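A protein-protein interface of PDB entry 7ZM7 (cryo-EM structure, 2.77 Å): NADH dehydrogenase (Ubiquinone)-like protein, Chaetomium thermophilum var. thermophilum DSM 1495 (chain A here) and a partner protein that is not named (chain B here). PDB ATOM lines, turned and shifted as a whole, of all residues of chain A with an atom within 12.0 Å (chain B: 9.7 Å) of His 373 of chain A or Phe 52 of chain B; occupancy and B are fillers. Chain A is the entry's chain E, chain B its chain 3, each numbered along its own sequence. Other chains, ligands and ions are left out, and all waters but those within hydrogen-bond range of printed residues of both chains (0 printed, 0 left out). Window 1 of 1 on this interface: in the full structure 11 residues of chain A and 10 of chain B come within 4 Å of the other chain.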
ATOM      1  N   SER A 360      -3.861 -12.194  17.487  1.00  0.00           N
ATOM      2  CA  SER A 360      -2.802 -11.650  16.593  1.00  0.00           C
ATOM      3  C   SER A 360      -2.032 -10.474  17.198  1.00  0.00           C
ATOM      4  O   SER A 360      -2.567  -9.819  18.111  1.00  0.00           O
ATOM      5  CB  SER A 360      -3.376 -11.282  15.262  1.00  0.00           C
ATOM      6  OG  SER A 360      -4.402 -10.320  15.424  1.00  0.00           O
ATOM      7  N   THR A 361      -0.822 -10.222  16.685  1.00  0.00           N
ATOM      8  CA  THR A 361       0.022  -9.100  17.171  1.00  0.00           C
ATOM      9  C   THR A 361      -0.199  -7.864  16.300  1.00  0.00           C
ATOM     10  O   THR A 361      -0.729  -8.025  15.195  1.00  0.00           O
ATOM     11  CB  THR A 361       1.508  -9.463  17.110  1.00  0.00           C
ATOM     12  OG1 THR A 361       1.938  -9.338  15.753  1.00  0.00           O
ATOM     13  CG2 THR A 361       1.801 -10.853  17.627  1.00  0.00           C
ATOM     14  N   GLU A 362       0.241  -6.693  16.758  1.00  0.00           N
ATOM     15  CA  GLU A 362       0.043  -5.431  16.054  1.00  0.00           C
ATOM     16  C   GLU A 362       0.822  -5.394  14.743  1.00  0.00           C
ATOM     17  O   GLU A 362       0.395  -4.755  13.777  1.00  0.00           O
ATOM     18  CB  GLU A 362       0.439  -4.261  16.955  1.00  0.00           C
ATOM     19  CG  GLU A 362       1.920  -4.184  17.294  1.00  0.00           C
ATOM     20  CD  GLU A 362       2.675  -3.252  16.365  1.00  0.00           C
ATOM     21  OE1 GLU A 362       2.017  -2.440  15.684  1.00  0.00           O
ATOM     22  OE2 GLU A 362       3.920  -3.322  16.319  1.00  0.00           O
ATOM     23  N   LYS A 363       1.971  -6.066  14.693  1.00  0.00           N
ATOM     24  CA  LYS A 363       2.772  -6.043  13.476  1.00  0.00           C
ATOM     25  C   LYS A 363       2.038  -6.735  12.341  1.00  0.00           C
ATOM     26  O   LYS A 363       2.004  -6.237  11.210  1.00  0.00           O
ATOM     27  CB  LYS A 363       4.136  -6.693  13.730  1.00  0.00           C
ATOM     28  CG  LYS A 363       5.078  -6.701  12.526  1.00  0.00           C
ATOM     29  CD  LYS A 363       4.986  -7.984  11.712  1.00  0.00           C
ATOM     30  CE  LYS A 363       5.578  -9.165  12.458  1.00  0.00           C
ATOM     31  NZ  LYS A 363       5.500 -10.414  11.651  1.00  0.00           N
ATOM     32  N   GLU A 364       1.419  -7.881  12.643  1.00  0.00           N
ATOM     33  CA  GLU A 364       0.726  -8.656  11.580  1.00  0.00           C
ATOM     34  C   GLU A 364      -0.651  -8.049  11.302  1.00  0.00           C
ATOM     35  O   GLU A 364      -1.150  -8.238  10.183  1.00  0.00           O
ATOM     36  CB  GLU A 364       0.701 -10.154  11.894  1.00  0.00           C
ATOM     37  CG  GLU A 364       0.081 -10.502  13.231  1.00  0.00           C
ATOM     38  CD  GLU A 364       0.250 -11.960  13.623  1.00  0.00           C
ATOM     39  OE1 GLU A 364       0.539 -12.779  12.729  1.00  0.00           O
ATOM     40  OE2 GLU A 364       0.107 -12.271  14.820  1.00  0.00           O
ATOM     41  N   MET A 365      -1.235  -7.348  12.272  1.00  0.00           N
ATOM     42  CA  MET A 365      -2.526  -6.648  12.029  1.00  0.00           C
ATOM     43  C   MET A 365      -2.280  -5.598  10.948  1.00  0.00           C
ATOM     44  O   MET A 365      -3.177  -5.391  10.119  1.00  0.00           O
ATOM     45  CB  MET A 365      -3.036  -5.962  13.298  1.00  0.00           C
ATOM     46  CG  MET A 365      -3.701  -6.910  14.274  1.00  0.00           C
ATOM     47  SD  MET A 365      -5.231  -7.618  13.614  1.00  0.00           S
ATOM     48  CE  MET A 365      -6.233  -6.141  13.453  1.00  0.00           C
ATOM     49  N   ARG A 366      -1.118  -4.952  10.979  1.00  0.00           N
ATOM     50  CA  ARG A 366      -0.742  -3.958   9.940  1.00  0.00           C
ATOM     51  C   ARG A 366      -0.606  -4.648   8.582  1.00  0.00           C
ATOM     52  O   ARG A 366      -0.978  -4.030   7.574  1.00  0.00           O
ATOM     53  CB  ARG A 366       0.552  -3.238  10.336  1.00  0.00           C
ATOM     54  CG  ARG A 366       0.387  -2.293  11.517  1.00  0.00           C
ATOM     55  CD  ARG A 366       1.685  -1.625  11.928  1.00  0.00           C
ATOM     56  NE  ARG A 366       2.669  -2.567  12.443  1.00  0.00           N
ATOM     57  CZ  ARG A 366       3.867  -2.221  12.898  1.00  0.00           C
ATOM     58  NH1 ARG A 366       4.229  -0.949  12.905  1.00  0.00           N
ATOM     59  NH2 ARG A 366       4.698  -3.142  13.349  1.00  0.00           N
ATOM     60  N   GLU A 367      -0.075  -5.869   8.555  1.00  0.00           N
ATOM     61  CA  GLU A 367       0.164  -6.592   7.277  1.00  0.00           C
ATOM     62  C   GLU A 367      -1.172  -6.804   6.568  1.00  0.00           C
ATOM     63  O   GLU A 367      -1.197  -6.710   5.330  1.00  0.00           O
ATOM     64  CB  GLU A 367       0.890  -7.914   7.527  1.00  0.00           C
ATOM     65  CG  GLU A 367       2.225  -7.744   8.225  1.00  0.00           C
ATOM     66  CD  GLU A 367       3.260  -6.944   7.454  1.00  0.00           C
ATOM     67  OE1 GLU A 367       3.328  -7.101   6.218  1.00  0.00           O
ATOM     68  OE2 GLU A 367       3.992  -6.160   8.090  1.00  0.00           O
ATOM     69  N   GLU A 368      -2.241  -6.977   7.346  1.00  0.00           N
ATOM     70  CA  GLU A 368      -3.587  -7.223   6.778  1.00  0.00           C
ATOM     71  C   GLU A 368      -4.073  -5.977   6.034  1.00  0.00           C
ATOM     72  O   GLU A 368      -4.958  -6.117   5.199  1.00  0.00           O
ATOM     73  CB  GLU A 368      -4.543  -7.661   7.887  1.00  0.00           C
ATOM     74  CG  GLU A 368      -4.020  -8.813   8.721  1.00  0.00           C
ATOM     75  CD  GLU A 368      -3.874 -10.149   8.012  1.00  0.00           C
ATOM     76  OE1 GLU A 368      -3.026 -10.952   8.446  1.00  0.00           O
ATOM     77  OE2 GLU A 368      -4.616 -10.395   7.043  1.00  0.00           O
ATOM     78  N   ARG A 369      -3.479  -4.807   6.263  1.00  0.00           N
ATOM     79  CA  ARG A 369      -4.028  -3.600   5.595  1.00  0.00           C
ATOM     80  C   ARG A 369      -3.454  -3.500   4.181  1.00  0.00           C
ATOM     81  O   ARG A 369      -3.874  -2.612   3.444  1.00  0.00           O
ATOM     82  CB  ARG A 369      -3.766  -2.339   6.420  1.00  0.00           C
ATOM     83  CG  ARG A 369      -4.217  -2.429   7.871  1.00  0.00           C
ATOM     84  CD  ARG A 369      -5.718  -2.545   8.057  1.00  0.00           C
ATOM     85  NE  ARG A 369      -6.050  -2.363   9.462  1.00  0.00           N
ATOM     86  CZ  ARG A 369      -6.140  -3.347  10.347  1.00  0.00           C
ATOM     87  NH1 ARG A 369      -5.944  -4.599   9.972  1.00  0.00           N
ATOM     88  NH2 ARG A 369      -6.431  -3.077  11.607  1.00  0.00           N
ATOM     89  N   LYS A 370      -2.512  -4.372   3.824  1.00  0.00           N
ATOM     90  CA  LYS A 370      -2.017  -4.382   2.421  1.00  0.00           C
ATOM     91  C   LYS A 370      -2.809  -5.370   1.574  1.00  0.00           C
ATOM     92  O   LYS A 370      -2.522  -5.435   0.386  1.00  0.00           O
ATOM     93  CB  LYS A 370      -0.548  -4.804   2.395  1.00  0.00           C
ATOM     94  CG  LYS A 370       0.327  -4.148   3.453  1.00  0.00           C
ATOM     95  CD  LYS A 370       1.709  -4.754   3.551  1.00  0.00           C
ATOM     96  CE  LYS A 370       2.607  -4.020   4.523  1.00  0.00           C
ATOM     97  NZ  LYS A 370       2.031  -3.991   5.889  1.00  0.00           N
ATOM     98  N   TYR A 371      -3.785  -6.070   2.143  1.00  0.00           N
ATOM     99  CA  TYR A 371      -4.618  -6.958   1.354  1.00  0.00           C
ATOM    100  C   TYR A 371      -6.058  -6.478   1.357  1.00  0.00           C
ATOM    101  O   TYR A 371      -6.503  -5.799   2.280  1.00  0.00           O
ATOM    102  CB  TYR A 371      -4.563  -8.384   1.890  1.00  0.00           C
ATOM    103  CG  TYR A 371      -3.235  -9.050   1.686  1.00  0.00           C
ATOM    104  CD1 TYR A 371      -2.227  -8.922   2.621  1.00  0.00           C
ATOM    105  CD2 TYR A 371      -2.981  -9.787   0.555  1.00  0.00           C
ATOM    106  CE1 TYR A 371      -1.021  -9.519   2.442  1.00  0.00           C
ATOM    107  CE2 TYR A 371      -1.776 -10.388   0.370  1.00  0.00           C
ATOM    108  CZ  TYR A 371      -0.797 -10.253   1.318  1.00  0.00           C
ATOM    109  OH  TYR A 371       0.419 -10.849   1.124  1.00  0.00           O
ATOM    110  N   LEU A 372      -6.788  -6.854   0.310  1.00  0.00           N
ATOM    111  CA  LEU A 372      -8.254  -6.654   0.314  1.00  0.00           C
ATOM    112  C   LEU A 372      -8.794  -8.024   0.746  1.00  0.00           C
ATOM    113  O   LEU A 372      -8.331  -9.034   0.195  1.00  0.00           O
ATOM    114  CB  LEU A 372      -8.706  -6.249  -1.091  1.00  0.00           C
ATOM    115  CG  LEU A 372      -8.827  -4.747  -1.340  1.00  0.00           C
ATOM    116  CD1 LEU A 372      -9.289  -4.469  -2.761  1.00  0.00           C
ATOM    117  CD2 LEU A 372      -9.778  -4.110  -0.340  1.00  0.00           C
ATOM    118  N   HIS A 373      -9.701  -8.078   1.713  1.00  0.00           N
ATOM    119  CA  HIS A 373     -10.150  -9.382   2.262  1.00  0.00           C
ATOM    120  C   HIS A 373     -11.512  -9.752   1.686  1.00  0.00           C
ATOM    121  O   HIS A 373     -12.088 -10.756   2.127  1.00  0.00           O
ATOM    122  CB  HIS A 373     -10.135  -9.285   3.790  1.00  0.00           C
ATOM    123  CG  HIS A 373      -8.816  -8.844   4.314  1.00  0.00           C
ATOM    124  ND1 HIS A 373      -7.837  -9.739   4.686  1.00  0.00           N
ATOM    125  CD2 HIS A 373      -8.303  -7.614   4.509  1.00  0.00           C
ATOM    126  CE1 HIS A 373      -6.781  -9.078   5.103  1.00  0.00           C
ATOM    127  NE2 HIS A 373      -7.046  -7.779   5.007  1.00  0.00           N
ATOM    128  N   VAL A 374     -11.985  -8.969   0.724  1.00  0.00           N
ATOM    129  CA  VAL A 374     -13.268  -9.280   0.042  1.00  0.00           C
ATOM    130  C   VAL A 374     -13.073  -9.101  -1.455  1.00  0.00           C
ATOM    131  O   VAL A 374     -12.279  -8.240  -1.823  1.00  0.00           O
ATOM    132  CB  VAL A 374     -14.453  -8.452   0.587  1.00  0.00           C
ATOM    133  CG1 VAL A 374     -15.715  -8.594  -0.252  1.00  0.00           C
ATOM    134  CG2 VAL A 374     -14.748  -8.774   2.042  1.00  0.00           C
ATOM    135  N   LEU A 375     -13.694  -9.949  -2.264  1.00  0.00           N
ATOM    136  CA  LEU A 375     -13.694  -9.800  -3.715  1.00  0.00           C
ATOM    137  C   LEU A 375     -15.010  -9.174  -4.136  1.00  0.00           C
ATOM    138  O   LEU A 375     -16.024  -9.857  -4.255  1.00  0.00           O
ATOM    139  CB  LEU A 375     -13.478 -11.148  -4.386  1.00  0.00           C
ATOM    140  CG  LEU A 375     -12.089 -11.700  -4.133  1.00  0.00           C
ATOM    141  CD1 LEU A 375     -12.011 -13.099  -4.630  1.00  0.00           C
ATOM    142  CD2 LEU A 375     -11.073 -10.836  -4.821  1.00  0.00           C
ATOM    143  N   ASP A 376     -14.990  -7.869  -4.393  1.00  0.00           N
ATOM    144  CA  ASP A 376     -16.208  -7.124  -4.671  1.00  0.00           C
ATOM    145  C   ASP A 376     -16.682  -7.243  -6.114  1.00  0.00           C
ATOM    146  O   ASP A 376     -17.764  -6.746  -6.428  1.00  0.00           O
ATOM    147  CB  ASP A 376     -16.016  -5.654  -4.320  1.00  0.00           C
ATOM    148  CG  ASP A 376     -14.802  -5.047  -4.982  1.00  0.00           C
ATOM    149  OD1 ASP A 376     -14.014  -5.793  -5.600  1.00  0.00           O
ATOM    150  OD2 ASP A 376     -14.634  -3.817  -4.889  1.00  0.00           O
ATOM    151  N   ASP A 377     -15.922  -7.880  -6.985  1.00  0.00           N
ATOM    152  CA  ASP A 377     -16.333  -8.076  -8.364  1.00  0.00           C
ATOM    153  C   ASP A 377     -16.633  -9.528  -8.693  1.00  0.00           C
ATOM    154  O   ASP A 377     -16.925  -9.842  -9.848  1.00  0.00           O
ATOM    155  CB  ASP A 377     -15.276  -7.511  -9.314  1.00  0.00           C
ATOM    156  CG  ASP A 377     -13.953  -8.234  -9.220  1.00  0.00           C
ATOM    157  OD1 ASP A 377     -13.853  -9.233  -8.476  1.00  0.00           O
ATOM    158  OD2 ASP A 377     -13.001  -7.793  -9.897  1.00  0.00           O
ATOM    159  N   GLN A 378     -16.584 -10.408  -7.701  1.00  0.00           N
ATOM    160  CA  GLN A 378     -16.932 -11.805  -7.873  1.00  0.00           C
ATOM    161  C   GLN A 378     -18.039 -12.200  -6.911  1.00  0.00           C
ATOM    162  O   GLN A 378     -17.993 -11.871  -5.733  1.00  0.00           O
ATOM    163  CB  GLN A 378     -15.708 -12.692  -7.666  1.00  0.00           C
ATOM    164  CG  GLN A 378     -14.524 -12.299  -8.529  1.00  0.00           C
ATOM    165  CD  GLN A 378     -13.584 -13.450  -8.791  1.00  0.00           C
ATOM    166  OE1 GLN A 378     -14.014 -14.589  -8.990  1.00  0.00           O
ATOM    167  NE2 GLN A 378     -12.286 -13.163  -8.791  1.00  0.00           N
ATOM    168  N   SER B  48      -5.155 -20.603   6.581  1.00  0.00           N
ATOM    169  CA  SER B  48      -4.820 -19.701   5.489  1.00  0.00           C
ATOM    170  C   SER B  48      -5.958 -18.709   5.312  1.00  0.00           C
ATOM    171  O   SER B  48      -7.082 -18.940   5.764  1.00  0.00           O
ATOM    172  CB  SER B  48      -4.555 -20.463   4.187  1.00  0.00           C
ATOM    173  OG  SER B  48      -5.674 -21.254   3.824  1.00  0.00           O
ATOM    174  N   ARG B  49      -5.654 -17.601   4.643  1.00  0.00           N
ATOM    175  CA  ARG B  49      -6.641 -16.566   4.378  1.00  0.00           C
ATOM    176  C   ARG B  49      -6.814 -16.401   2.881  1.00  0.00           C
ATOM    177  O   ARG B  49      -5.832 -16.284   2.143  1.00  0.00           O
ATOM    178  CB  ARG B  49      -6.239 -15.225   4.989  1.00  0.00           C
ATOM    179  CG  ARG B  49      -6.032 -15.266   6.489  1.00  0.00           C
ATOM    180  CD  ARG B  49      -6.223 -13.891   7.074  1.00  0.00           C
ATOM    181  NE  ARG B  49      -7.522 -13.375   6.669  1.00  0.00           N
ATOM    182  CZ  ARG B  49      -8.026 -12.203   7.029  1.00  0.00           C
ATOM    183  NH1 ARG B  49      -7.340 -11.391   7.818  1.00  0.00           N
ATOM    184  NH2 ARG B  49      -9.225 -11.852   6.591  1.00  0.00           N
ATOM    185  N   SER B  50      -8.068 -16.406   2.433  1.00  0.00           N
ATOM    186  CA  SER B  50      -8.361 -16.009   1.075  1.00  0.00           C
ATOM    187  C   SER B  50      -9.606 -15.155   1.142  1.00  0.00           C
ATOM    188  O   SER B  50     -10.497 -15.444   1.948  1.00  0.00           O
ATOM    189  CB  SER B  50      -8.576 -17.187   0.121  1.00  0.00           C
ATOM    190  OG  SER B  50      -7.355 -17.854  -0.159  1.00  0.00           O
ATOM    191  N   PRO B  51      -9.688 -14.102   0.339  1.00  0.00           N
ATOM    192  CA  PRO B  51     -10.907 -13.293   0.319  1.00  0.00           C
ATOM    193  C   PRO B  51     -12.091 -14.135  -0.106  1.00  0.00           C
ATOM    194  O   PRO B  51     -11.980 -14.998  -0.977  1.00  0.00           O
ATOM    195  CB  PRO B  51     -10.600 -12.203  -0.714  1.00  0.00           C
ATOM    196  CG  PRO B  51      -9.158 -12.293  -0.985  1.00  0.00           C
ATOM    197  CD  PRO B  51      -8.723 -13.679  -0.681  1.00  0.00           C
ATOM    198  N   PHE B  52     -13.234 -13.876   0.505  1.00  0.00           N
ATOM    199  CA  PHE B  52     -14.465 -14.504   0.060  1.00  0.00           C
ATOM    200  C   PHE B  52     -15.149 -13.618  -0.965  1.00  0.00           C
ATOM    201  O   PHE B  52     -15.029 -12.392  -0.936  1.00  0.00           O
ATOM    202  CB  PHE B  52     -15.401 -14.795   1.240  1.00  0.00           C
ATOM    203  CG  PHE B  52     -16.122 -13.592   1.778  1.00  0.00           C
ATOM    204  CD1 PHE B  52     -15.532 -12.782   2.709  1.00  0.00           C
ATOM    205  CD2 PHE B  52     -17.411 -13.312   1.386  1.00  0.00           C
ATOM    206  CE1 PHE B  52     -16.198 -11.699   3.209  1.00  0.00           C
ATOM    207  CE2 PHE B  52     -18.084 -12.220   1.881  1.00  0.00           C
ATOM    208  CZ  PHE B  52     -17.482 -11.416   2.795  1.00  0.00           C
ATOM    209  N   ASN B  53     -15.848 -14.258  -1.892  1.00  0.00           N
ATOM    210  CA  ASN B  53     -16.507 -13.542  -2.972  1.00  0.00           C
ATOM    211  C   ASN B  53     -17.745 -12.824  -2.458  1.00  0.00           C
ATOM    212  O   ASN B  53     -18.469 -13.337  -1.603  1.00  0.00           O
ATOM    213  CB  ASN B  53     -16.860 -14.515  -4.089  1.00  0.00           C
ATOM    214  CG  ASN B  53     -15.701 -15.437  -4.426  1.00  0.00           C
ATOM    215  OD1 ASN B  53     -14.723 -15.017  -5.038  1.00  0.00           O
ATOM    216  ND2 ASN B  53     -15.793 -16.698  -4.000  1.00  0.00           N
ATOM    217  N   ILE B  54     -17.986 -11.617  -2.972  1.00  0.00           N
ATOM    218  CA  ILE B  54     -19.088 -10.831  -2.442  1.00  0.00           C
ATOM    219  C   ILE B  54     -20.435 -11.376  -2.884  1.00  0.00           C
ATOM    220  O   ILE B  54     -21.452 -11.082  -2.257  1.00  0.00           O
ATOM    221  CB  ILE B  54     -18.924  -9.339  -2.804  1.00  0.00           C
ATOM    222  CG1 ILE B  54     -19.886  -8.499  -1.974  1.00  0.00           C
ATOM    223  CG2 ILE B  54     -19.196  -9.112  -4.261  1.00  0.00           C
ATOM    224  CD1 ILE B  54     -19.653  -8.614  -0.527  1.00  0.00           C
ATOM    225  N   SER B  55     -20.462 -12.206  -3.921  1.00  0.00           N
ATOM    226  CA  SER B  55     -21.727 -12.681  -4.461  1.00  0.00           C
ATOM    227  C   SER B  55     -22.464 -13.578  -3.479  1.00  0.00           C
ATOM    228  O   SER B  55     -23.692 -13.681  -3.539  1.00  0.00           O
ATOM    229  CB  SER B  55     -21.484 -13.400  -5.788  1.00  0.00           C
ATOM    230  OG  SER B  55     -20.683 -14.544  -5.614  1.00  0.00           O
ATOM    231  N   PHE B  56     -21.742 -14.227  -2.564  1.00  0.00           N
ATOM    232  CA  PHE B  56     -22.397 -14.974  -1.495  1.00  0.00           C
ATOM    233  C   PHE B  56     -23.266 -14.067  -0.643  1.00  0.00           C
ATOM    234  O   PHE B  56     -24.376 -14.439  -0.254  1.00  0.00           O
ATOM    235  CB  PHE B  56     -21.360 -15.666  -0.626  1.00  0.00           C
ATOM    236  CG  PHE B  56     -20.839 -16.921  -1.217  1.00  0.00           C
ATOM    237  CD1 PHE B  56     -21.713 -17.907  -1.632  1.00  0.00           C
ATOM    238  CD2 PHE B  56     -19.481 -17.120  -1.368  1.00  0.00           C
ATOM    239  CE1 PHE B  56     -21.245 -19.054  -2.188  1.00  0.00           C
ATOM    240  CE2 PHE B  56     -19.005 -18.275  -1.928  1.00  0.00           C
ATOM    241  CZ  PHE B  56     -19.889 -19.245  -2.332  1.00  0.00           C
ATOM    242  N   PHE B  57     -22.768 -12.879  -0.322  1.00  0.00           N
ATOM    243  CA  PHE B  57     -23.565 -11.933   0.437  1.00  0.00           C
ATOM    244  C   PHE B  57     -24.796 -11.516  -0.346  1.00  0.00           C
ATOM    245  O   PHE B  57     -25.890 -11.417   0.213  1.00  0.00           O
ATOM    246  CB  PHE B  57     -22.710 -10.724   0.823  1.00  0.00           C
ATOM    247  CG  PHE B  57     -23.482  -9.638   1.469  1.00  0.00           C
ATOM    248  CD1 PHE B  57     -24.061  -9.835   2.707  1.00  0.00           C
ATOM    249  CD2 PHE B  57     -23.672  -8.433   0.832  1.00  0.00           C
ATOM    250  CE1 PHE B  57     -24.804  -8.849   3.299  1.00  0.00           C
ATOM    251  CE2 PHE B  57     -24.403  -7.450   1.417  1.00  0.00           C
ATOM    252  CZ  PHE B  57     -24.972  -7.662   2.656  1.00  0.00           C
ATOM    253  N   ILE B  58     -24.642 -11.288  -1.646  1.00  0.00           N
ATOM    254  CA  ILE B  58     -25.744 -10.790  -2.458  1.00  0.00           C
ATOM    255  C   ILE B  58     -26.842 -11.837  -2.590  1.00  0.00           C
ATOM    256  O   ILE B  58     -28.026 -11.504  -2.645  1.00  0.00           O
ATOM    257  CB  ILE B  58     -25.223 -10.329  -3.829  1.00  0.00           C
ATOM    258  CG1 ILE B  58     -23.973  -9.453  -3.670  1.00  0.00           C
ATOM    259  CG2 ILE B  58     -26.319  -9.619  -4.610  1.00  0.00           C
ATOM    260  CD1 ILE B  58     -24.118  -8.323  -2.737  1.00  0.00           C
ATOM    261  N   TYR B  59     -26.477 -13.114  -2.655  1.00  0.00           N
ATOM    262  CA  TYR B  59     -27.481 -14.168  -2.719  1.00  0.00           C
ATOM    263  C   TYR B  59     -28.374 -14.145  -1.490  1.00  0.00           C
ATOM    264  O   TYR B  59     -29.600 -14.210  -1.601  1.00  0.00           O
ATOM    265  CB  TYR B  59     -26.799 -15.527  -2.870  1.00  0.00           C
ATOM    266  CG  TYR B  59     -26.116 -15.695  -4.194  1.00  0.00           C
ATOM    267  CD1 TYR B  59     -26.494 -14.944  -5.276  1.00  0.00           C
ATOM    268  CD2 TYR B  59     -25.025 -16.539  -4.337  1.00  0.00           C
ATOM    269  CE1 TYR B  59     -25.866 -15.071  -6.476  1.00  0.00           C
ATOM    270  CE2 TYR B  59     -24.382 -16.661  -5.539  1.00  0.00           C
ATOM    271  CZ  TYR B  59     -24.814 -15.925  -6.602  1.00  0.00           C
ATOM    272  OH  TYR B  59     -24.188 -16.028  -7.817  1.00  0.00           O
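Tyr 371 of chain A touches none of the printed residues of chain B.
Of the printed residues of chain B, Leu 372 of chain A touches Pro 51 (3.6 Å).
His 373 of chain A touches three residues of chain B.
Val 374 of chain A touches three residues of chain B.
Of the printed residues of chain B, Leu 375 of chain A touches Pro 51 (3.8 Å), Phe 52 (3.1 Å), Asn 53 (3.3 Å) and Ile 54 (2.9 Å).
Of the printed residues of chain B, Asp 376 of chain A touches Ile 54.
Of chain A, only His 373, Val 374 and Leu 375 come within 4 Å of Phe 52 of chain B.
Printed residues of chain A within 4 Å of Asn 53 of chain B: Leu 375 (3.3 Å) and Gln 378 (3.3 Å).
Ile 54 of chain B touches just these residues of chain A: Val 374 (3.9 Å), Leu 375 (2.9 Å), Asp 376 (3.5 Å) and Gln 378 (2.8 Å).
No residue of chain A comes within 4 Å of Phe 56 of chain B.
The nearest residue of chain B that does not touch His 373 of chain A is Ser 50 of chain B (5.0 Å).
The nearest residue of chain A that does not touch Phe 52 of chain B is Gln 378 of chain A (5.7 Å).
Hydrophobic or aromatic side chains of chain B that line the printed part of chain A: Pro 51, Phe 52 and Ile 54.
Printed residues of chain A that touch a printed residue of chain B: Glu 368, Leu 372, His 373, Val 374, Leu 375, Asp 376 and Gln 378.
Hydrophobic or aromatic side chains of chain A within 4 Å of the printed part of chain B: His 373, Val 374 and Leu 375.
Among the printed residues, Asp or Glu carboxylates within 4 Å of a Lys or Arg side-chain nitrogen of the other chain: Glu 368 of chain A with Arg 49 of chain B (3.0 Å).
The backbone carbonyl oxygen (O) of Phe 52 of chain B lies within hydrogen-bond range of the backbone NH (N) of Leu 375 of chain A, 3.1 Å away.
The side-chain carboxylate (OE2) of Glu 368 of chain A is in salt-bridge range of the guanidinium group (NH1) of Arg 49 of chain B (3.0 Å).
The backbone carbonyl oxygen (O) of Gln 378 of chain A sits at hydrogen-bond distance from the backbone NH (N) of Ile 54 of chain B (2.8 Å).
The backbone carbonyl oxygen (O) of Leu 375 of chain A lies within hydrogen-bond range of the backbone NH (N) of Ile 54 of chain B (2.9 Å).
The backbone NH (N) of Ser 55 of chain B is in hydrogen-bond range of the backbone carbonyl oxygen (O) of Gln 378 of chain A (3.1 Å).
The guanidinium group of Arg 49 of chain B sits at hydrogen-bond distance from a ring nitrogen (ND1) of His 373 of chain A, 3.2 Å away.
The backbone carbonyl oxygen of Glu 368 of chain A is in hydrogen-bond range of a ring nitrogen (NE2) of His 373 of chain A.
A ring nitrogen (NE2) of His 373 of chain A sits close to the backbone carbonyl oxygen of Tyr 371 of chain A (3.4 Å).
Among the printed residues, pairs that only touch across the chains: Gln 378 of chain A with Asn 53 of chain B (3.3 Å), His 373 of chain A with Pro 51 of chain B (3.3 Å), Leu 375 of chain A with Asn 53 of chain B (3.3 Å), Val 374 of chain A with Phe 52 of chain B (3.5 Å), Asp 376 of chain A with Ile 54 of chain B (3.5 Å), Leu 372 of chain A with Pro 51 of chain B (3.6 Å), His 373 of chain A with Phe 52 of chain B (3.7 Å), Leu 375 of chain A with Pro 51 of chain B (3.8 Å), Val 374 of chain A with Pro 51 of chain B (3.8 Å) and Val 374 of chain A with Ile 54 of chain B (3.9 Å).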
